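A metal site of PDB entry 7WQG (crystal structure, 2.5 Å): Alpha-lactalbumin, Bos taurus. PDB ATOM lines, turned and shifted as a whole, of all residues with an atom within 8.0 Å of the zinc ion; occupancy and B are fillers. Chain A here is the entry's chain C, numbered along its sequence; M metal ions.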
ATOM      1  N   GLU A  11     -24.851  -1.926   4.358  1.00  0.00           N
ATOM      2  CA  GLU A  11     -23.875  -0.888   4.068  1.00  0.00           C
ATOM      3  C   GLU A  11     -24.520   0.454   3.766  1.00  0.00           C
ATOM      4  O   GLU A  11     -23.851   1.486   3.885  1.00  0.00           O
ATOM      5  CB  GLU A  11     -22.998  -1.340   2.909  1.00  0.00           C
ATOM      6  CG  GLU A  11     -22.151  -2.514   3.291  1.00  0.00           C
ATOM      7  CD  GLU A  11     -21.079  -2.825   2.291  1.00  0.00           C
ATOM      8  OE1 GLU A  11     -20.744  -4.017   2.143  1.00  0.00           O
ATOM      9  OE2 GLU A  11     -20.573  -1.880   1.649  1.00  0.00           O
ATOM     10  N   THR A  38     -20.293  -2.300  -6.990  1.00  0.00           N
ATOM     11  CA  THR A  38     -19.714  -1.056  -6.508  1.00  0.00           C
ATOM     12  C   THR A  38     -18.546  -0.576  -7.352  1.00  0.00           C
ATOM     13  O   THR A  38     -18.098   0.568  -7.166  1.00  0.00           O
ATOM     14  CB  THR A  38     -19.249  -1.233  -5.065  1.00  0.00           C
ATOM     15  OG1 THR A  38     -17.911  -1.730  -5.049  1.00  0.00           O
ATOM     16  CG2 THR A  38     -20.161  -2.198  -4.331  1.00  0.00           C
ATOM     17  N   GLN A  39     -18.032  -1.404  -8.260  1.00  0.00           N
ATOM     18  CA  GLN A  39     -16.897  -1.071  -9.099  1.00  0.00           C
ATOM     19  C   GLN A  39     -17.277  -0.815 -10.532  1.00  0.00           C
ATOM     20  O   GLN A  39     -16.408  -0.814 -11.405  1.00  0.00           O
ATOM     21  CB  GLN A  39     -15.888  -2.209  -9.091  1.00  0.00           C
ATOM     22  CG  GLN A  39     -15.056  -2.325  -7.896  1.00  0.00           C
ATOM     23  CD  GLN A  39     -13.914  -3.231  -8.184  1.00  0.00           C
ATOM     24  OE1 GLN A  39     -13.776  -3.721  -9.290  1.00  0.00           O
ATOM     25  NE2 GLN A  39     -13.076  -3.465  -7.186  1.00  0.00           N
ATOM     26  N   GLY A  51     -19.891   3.283  -9.877  1.00  0.00           N
ATOM     27  CA  GLY A  51     -20.191   2.593  -8.636  1.00  0.00           C
ATOM     28  C   GLY A  51     -21.644   2.202  -8.432  1.00  0.00           C
ATOM     29  O   GLY A  51     -22.484   2.269  -9.328  1.00  0.00           O
ATOM     30  N   LEU A  52     -21.927   1.805  -7.196  1.00  0.00           N
ATOM     31  CA  LEU A  52     -23.232   1.231  -6.851  1.00  0.00           C
ATOM     32  C   LEU A  52     -24.377   2.169  -7.233  1.00  0.00           C
ATOM     33  O   LEU A  52     -25.445   1.705  -7.652  1.00  0.00           O
ATOM     34  CB  LEU A  52     -23.264   0.892  -5.359  1.00  0.00           C
ATOM     35  CG  LEU A  52     -24.538   0.336  -4.740  1.00  0.00           C
ATOM     36  CD1 LEU A  52     -24.943  -0.900  -5.459  1.00  0.00           C
ATOM     37  CD2 LEU A  52     -24.331   0.055  -3.278  1.00  0.00           C
ATOM     38  N   PHE A  53     -24.167   3.479  -7.105  1.00  0.00           N
ATOM     39  CA  PHE A  53     -25.174   4.459  -7.497  1.00  0.00           C
ATOM     40  C   PHE A  53     -24.892   5.105  -8.839  1.00  0.00           C
ATOM     41  O   PHE A  53     -25.734   5.852  -9.337  1.00  0.00           O
ATOM     42  CB  PHE A  53     -25.307   5.550  -6.450  1.00  0.00           C
ATOM     43  CG  PHE A  53     -25.568   5.039  -5.083  1.00  0.00           C
ATOM     44  CD1 PHE A  53     -26.853   4.917  -4.618  1.00  0.00           C
ATOM     45  CD2 PHE A  53     -24.514   4.688  -4.260  1.00  0.00           C
ATOM     46  CE1 PHE A  53     -27.091   4.447  -3.351  1.00  0.00           C
ATOM     47  CE2 PHE A  53     -24.749   4.221  -2.985  1.00  0.00           C
ATOM     48  CZ  PHE A  53     -26.038   4.105  -2.532  1.00  0.00           C
ATOM     49  N   ILE A  75     -15.037  15.503  -4.386  1.00  0.00           N
ATOM     50  CA  ILE A  75     -14.396  14.216  -4.235  1.00  0.00           C
ATOM     51  C   ILE A  75     -13.906  13.736  -5.588  1.00  0.00           C
ATOM     52  O   ILE A  75     -14.568  13.931  -6.616  1.00  0.00           O
ATOM     53  CB  ILE A  75     -15.371  13.196  -3.605  1.00  0.00           C
ATOM     54  CG1 ILE A  75     -14.665  11.890  -3.260  1.00  0.00           C
ATOM     55  CG2 ILE A  75     -16.572  12.958  -4.510  1.00  0.00           C
ATOM     56  CD1 ILE A  75     -15.579  10.886  -2.613  1.00  0.00           C
ATOM     57  N   CYS A  77     -13.570  11.120  -8.323  1.00  0.00           N
ATOM     58  CA  CYS A  77     -14.669  10.231  -8.654  1.00  0.00           C
ATOM     59  C   CYS A  77     -14.370   8.781  -8.309  1.00  0.00           C
ATOM     60  O   CYS A  77     -15.271   8.032  -7.944  1.00  0.00           O
ATOM     61  CB  CYS A  77     -14.980  10.388 -10.136  1.00  0.00           C
ATOM     62  SG  CYS A  77     -16.692  10.213 -10.412  1.00  0.00           S
ATOM     63  N   ASP A  78     -13.112   8.366  -8.392  1.00  0.00           N
ATOM     64  CA  ASP A  78     -12.780   6.948  -8.272  1.00  0.00           C
ATOM     65  C   ASP A  78     -12.904   6.409  -6.868  1.00  0.00           C
ATOM     66  O   ASP A  78     -12.684   5.214  -6.670  1.00  0.00           O
ATOM     67  CB  ASP A  78     -11.376   6.728  -8.789  1.00  0.00           C
ATOM     68  CG  ASP A  78     -10.392   7.701  -8.197  1.00  0.00           C
ATOM     69  OD1 ASP A  78     -10.785   8.458  -7.288  1.00  0.00           O
ATOM     70  OD2 ASP A  78      -9.229   7.720  -8.649  1.00  0.00           O
ATOM     71  N   LYS A  79     -13.223   7.234  -5.886  1.00  0.00           N
ATOM     72  CA  LYS A  79     -13.455   6.691  -4.552  1.00  0.00           C
ATOM     73  C   LYS A  79     -14.856   6.117  -4.395  1.00  0.00           C
ATOM     74  O   LYS A  79     -15.200   5.637  -3.310  1.00  0.00           O
ATOM     75  CB  LYS A  79     -13.197   7.780  -3.505  1.00  0.00           C
ATOM     76  CG  LYS A  79     -11.897   8.549  -3.735  1.00  0.00           C
ATOM     77  CD  LYS A  79     -11.188   8.859  -2.425  1.00  0.00           C
ATOM     78  CE  LYS A  79     -12.108   9.629  -1.480  1.00  0.00           C
ATOM     79  NZ  LYS A  79     -11.685   9.585  -0.044  1.00  0.00           N
ATOM     80  N   PHE A  80     -15.666   6.185  -5.449  1.00  0.00           N
ATOM     81  CA  PHE A  80     -16.884   5.397  -5.567  1.00  0.00           C
ATOM     82  C   PHE A  80     -16.630   4.037  -6.188  1.00  0.00           C
ATOM     83  O   PHE A  80     -17.583   3.302  -6.446  1.00  0.00           O
ATOM     84  CB  PHE A  80     -17.924   6.127  -6.422  1.00  0.00           C
ATOM     85  CG  PHE A  80     -18.130   7.552  -6.054  1.00  0.00           C
ATOM     86  CD1 PHE A  80     -18.161   7.937  -4.728  1.00  0.00           C
ATOM     87  CD2 PHE A  80     -18.308   8.511  -7.028  1.00  0.00           C
ATOM     88  CE1 PHE A  80     -18.344   9.248  -4.386  1.00  0.00           C
ATOM     89  CE2 PHE A  80     -18.495   9.819  -6.695  1.00  0.00           C
ATOM     90  CZ  PHE A  80     -18.520  10.191  -5.378  1.00  0.00           C
ATOM     91  N   LEU A  81     -15.377   3.705  -6.465  1.00  0.00           N
ATOM     92  CA  LEU A  81     -15.028   2.414  -7.044  1.00  0.00           C
ATOM     93  C   LEU A  81     -14.473   1.418  -6.041  1.00  0.00           C
ATOM     94  O   LEU A  81     -14.266   0.264  -6.389  1.00  0.00           O
ATOM     95  CB  LEU A  81     -14.015   2.617  -8.173  1.00  0.00           C
ATOM     96  CG  LEU A  81     -14.500   3.535  -9.288  1.00  0.00           C
ATOM     97  CD1 LEU A  81     -13.545   3.464 -10.448  1.00  0.00           C
ATOM     98  CD2 LEU A  81     -15.901   3.158  -9.712  1.00  0.00           C
ATOM     99  N   ASP A  82     -14.234   1.841  -4.807  1.00  0.00           N
ATOM    100  CA  ASP A  82     -13.809   0.908  -3.799  1.00  0.00           C
ATOM    101  C   ASP A  82     -15.026   0.355  -3.046  1.00  0.00           C
ATOM    102  O   ASP A  82     -16.175   0.672  -3.363  1.00  0.00           O
ATOM    103  CB  ASP A  82     -12.845   1.580  -2.841  1.00  0.00           C
ATOM    104  CG  ASP A  82     -13.512   2.633  -2.008  1.00  0.00           C
ATOM    105  OD1 ASP A  82     -14.689   2.953  -2.281  1.00  0.00           O
ATOM    106  OD2 ASP A  82     -12.860   3.123  -1.073  1.00  0.00           O
ATOM    107  N   ASP A  83     -14.750  -0.428  -2.023  1.00  0.00           N
ATOM    108  CA  ASP A  83     -15.773  -1.167  -1.302  1.00  0.00           C
ATOM    109  C   ASP A  83     -16.411  -0.369  -0.191  1.00  0.00           C
ATOM    110  O   ASP A  83     -17.514  -0.708   0.246  1.00  0.00           O
ATOM    111  CB  ASP A  83     -15.173  -2.437  -0.716  1.00  0.00           C
ATOM    112  CG  ASP A  83     -14.464  -3.257  -1.767  1.00  0.00           C
ATOM    113  OD1 ASP A  83     -13.264  -3.555  -1.588  1.00  0.00           O
ATOM    114  OD2 ASP A  83     -15.107  -3.574  -2.786  1.00  0.00           O
ATOM    115  N   ASP A  84     -15.757   0.676   0.287  1.00  0.00           N
ATOM    116  CA  ASP A  84     -16.325   1.520   1.310  1.00  0.00           C
ATOM    117  C   ASP A  84     -17.311   2.481   0.671  1.00  0.00           C
ATOM    118  O   ASP A  84     -16.941   3.244  -0.228  1.00  0.00           O
ATOM    119  CB  ASP A  84     -15.228   2.269   2.048  1.00  0.00           C
ATOM    120  CG  ASP A  84     -15.718   2.875   3.302  1.00  0.00           C
ATOM    121  OD1 ASP A  84     -16.777   3.524   3.254  1.00  0.00           O
ATOM    122  OD2 ASP A  84     -15.066   2.681   4.334  1.00  0.00           O
ATOM    123  N   LEU A  85     -18.559   2.441   1.128  1.00  0.00           N
ATOM    124  CA  LEU A  85     -19.613   3.253   0.553  1.00  0.00           C
ATOM    125  C   LEU A  85     -19.989   4.459   1.417  1.00  0.00           C
ATOM    126  O   LEU A  85     -21.065   5.016   1.249  1.00  0.00           O
ATOM    127  CB  LEU A  85     -20.862   2.408   0.297  1.00  0.00           C
ATOM    128  CG  LEU A  85     -20.680   1.078  -0.419  1.00  0.00           C
ATOM    129  CD1 LEU A  85     -21.943   0.257  -0.286  1.00  0.00           C
ATOM    130  CD2 LEU A  85     -20.343   1.334  -1.863  1.00  0.00           C
ATOM    131  N   THR A  86     -19.128   4.863   2.336  1.00  0.00           N
ATOM    132  CA  THR A  86     -19.509   5.968   3.213  1.00  0.00           C
ATOM    133  C   THR A  86     -19.531   7.282   2.442  1.00  0.00           C
ATOM    134  O   THR A  86     -20.515   8.018   2.493  1.00  0.00           O
ATOM    135  CB  THR A  86     -18.581   6.056   4.415  1.00  0.00           C
ATOM    136  OG1 THR A  86     -18.175   4.744   4.819  1.00  0.00           O
ATOM    137  CG2 THR A  86     -19.305   6.707   5.563  1.00  0.00           C
ATOM    138  N   ASP A  87     -18.456   7.588   1.714  1.00  0.00           N
ATOM    139  CA  ASP A  87     -18.447   8.806   0.907  1.00  0.00           C
ATOM    140  C   ASP A  87     -19.449   8.706  -0.231  1.00  0.00           C
ATOM    141  O   ASP A  87     -20.140   9.678  -0.536  1.00  0.00           O
ATOM    142  CB  ASP A  87     -17.039   9.101   0.382  1.00  0.00           C
ATOM    143  CG  ASP A  87     -16.449   7.947  -0.400  1.00  0.00           C
ATOM    144  OD1 ASP A  87     -17.232   7.092  -0.871  1.00  0.00           O
ATOM    145  OD2 ASP A  87     -15.222   7.899  -0.551  1.00  0.00           O
ATOM    146  N   ASP A  88     -19.524   7.535  -0.871  1.00  0.00           N
ATOM    147  CA  ASP A  88     -20.601   7.210  -1.792  1.00  0.00           C
ATOM    148  C   ASP A  88     -21.928   7.693  -1.214  1.00  0.00           C
ATOM    149  O   ASP A  88     -22.779   8.231  -1.929  1.00  0.00           O
ATOM    150  CB  ASP A  88     -20.679   5.695  -2.068  1.00  0.00           C
ATOM    151  CG  ASP A  88     -19.489   5.145  -2.842  1.00  0.00           C
ATOM    152  OD1 ASP A  88     -18.373   5.133  -2.303  1.00  0.00           O
ATOM    153  OD2 ASP A  88     -19.696   4.682  -3.974  1.00  0.00           O
ATOM    154  N   ILE A  89     -22.095   7.500   0.090  1.00  0.00           N
ATOM    155  CA  ILE A  89     -23.328   7.906   0.749  1.00  0.00           C
ATOM    156  C   ILE A  89     -23.412   9.426   0.826  1.00  0.00           C
ATOM    157  O   ILE A  89     -24.433  10.026   0.467  1.00  0.00           O
ATOM    158  CB  ILE A  89     -23.425   7.256   2.135  1.00  0.00           C
ATOM    159  CG1 ILE A  89     -23.922   5.816   2.012  1.00  0.00           C
ATOM    160  CG2 ILE A  89     -24.363   8.040   3.026  1.00  0.00           C
ATOM    161  CD1 ILE A  89     -24.067   5.094   3.340  1.00  0.00           C
HETATM  162 ZN    ZN M   1     -16.873   3.591  -2.207  1.00  0.00          ZN
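The side-chain hydroxyl (OG1) of Thr 38 is in hydrogen-bond range of the backbone carbonyl oxygen (O) of Asp 82, at 3.4 Å. The side-chain carboxylate (OD1) of Asp 87 sits close to the side-chain carboxylate (OD1) of Asp 88 (2.7 Å). The side-chain hydroxyl (OG1) of Thr 86 is in hydrogen-bond range of the side-chain carboxylate (OD1) of Asp 84 (2.4 Å). NZ of Lys 79 lies within salt-bridge range of OD2 of Asp 87, at 3.95 Å.
Lys 79 touches the zinc ion (O to ZN, 2.9 Å). Phe 80 touches the zinc ion (CA to ZN, 3.8 Å). CA of Leu 85 touches the zinc ion, at 3.9 Å. OD1 of Asp 87 touches the zinc ion, 3.8 Å away. Of the 20 residues printed, 7 come within 4 Å of the zinc ion.
The zinc ion is bound by O of Asp 84 (2.0 Å). OD1 of Asp 88 is bound to the zinc ion (2.2 Å). The zinc ion is bound by OD1 of Asp 82 (2.3 Å). The zinc ion has three donor atoms within binding distance.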
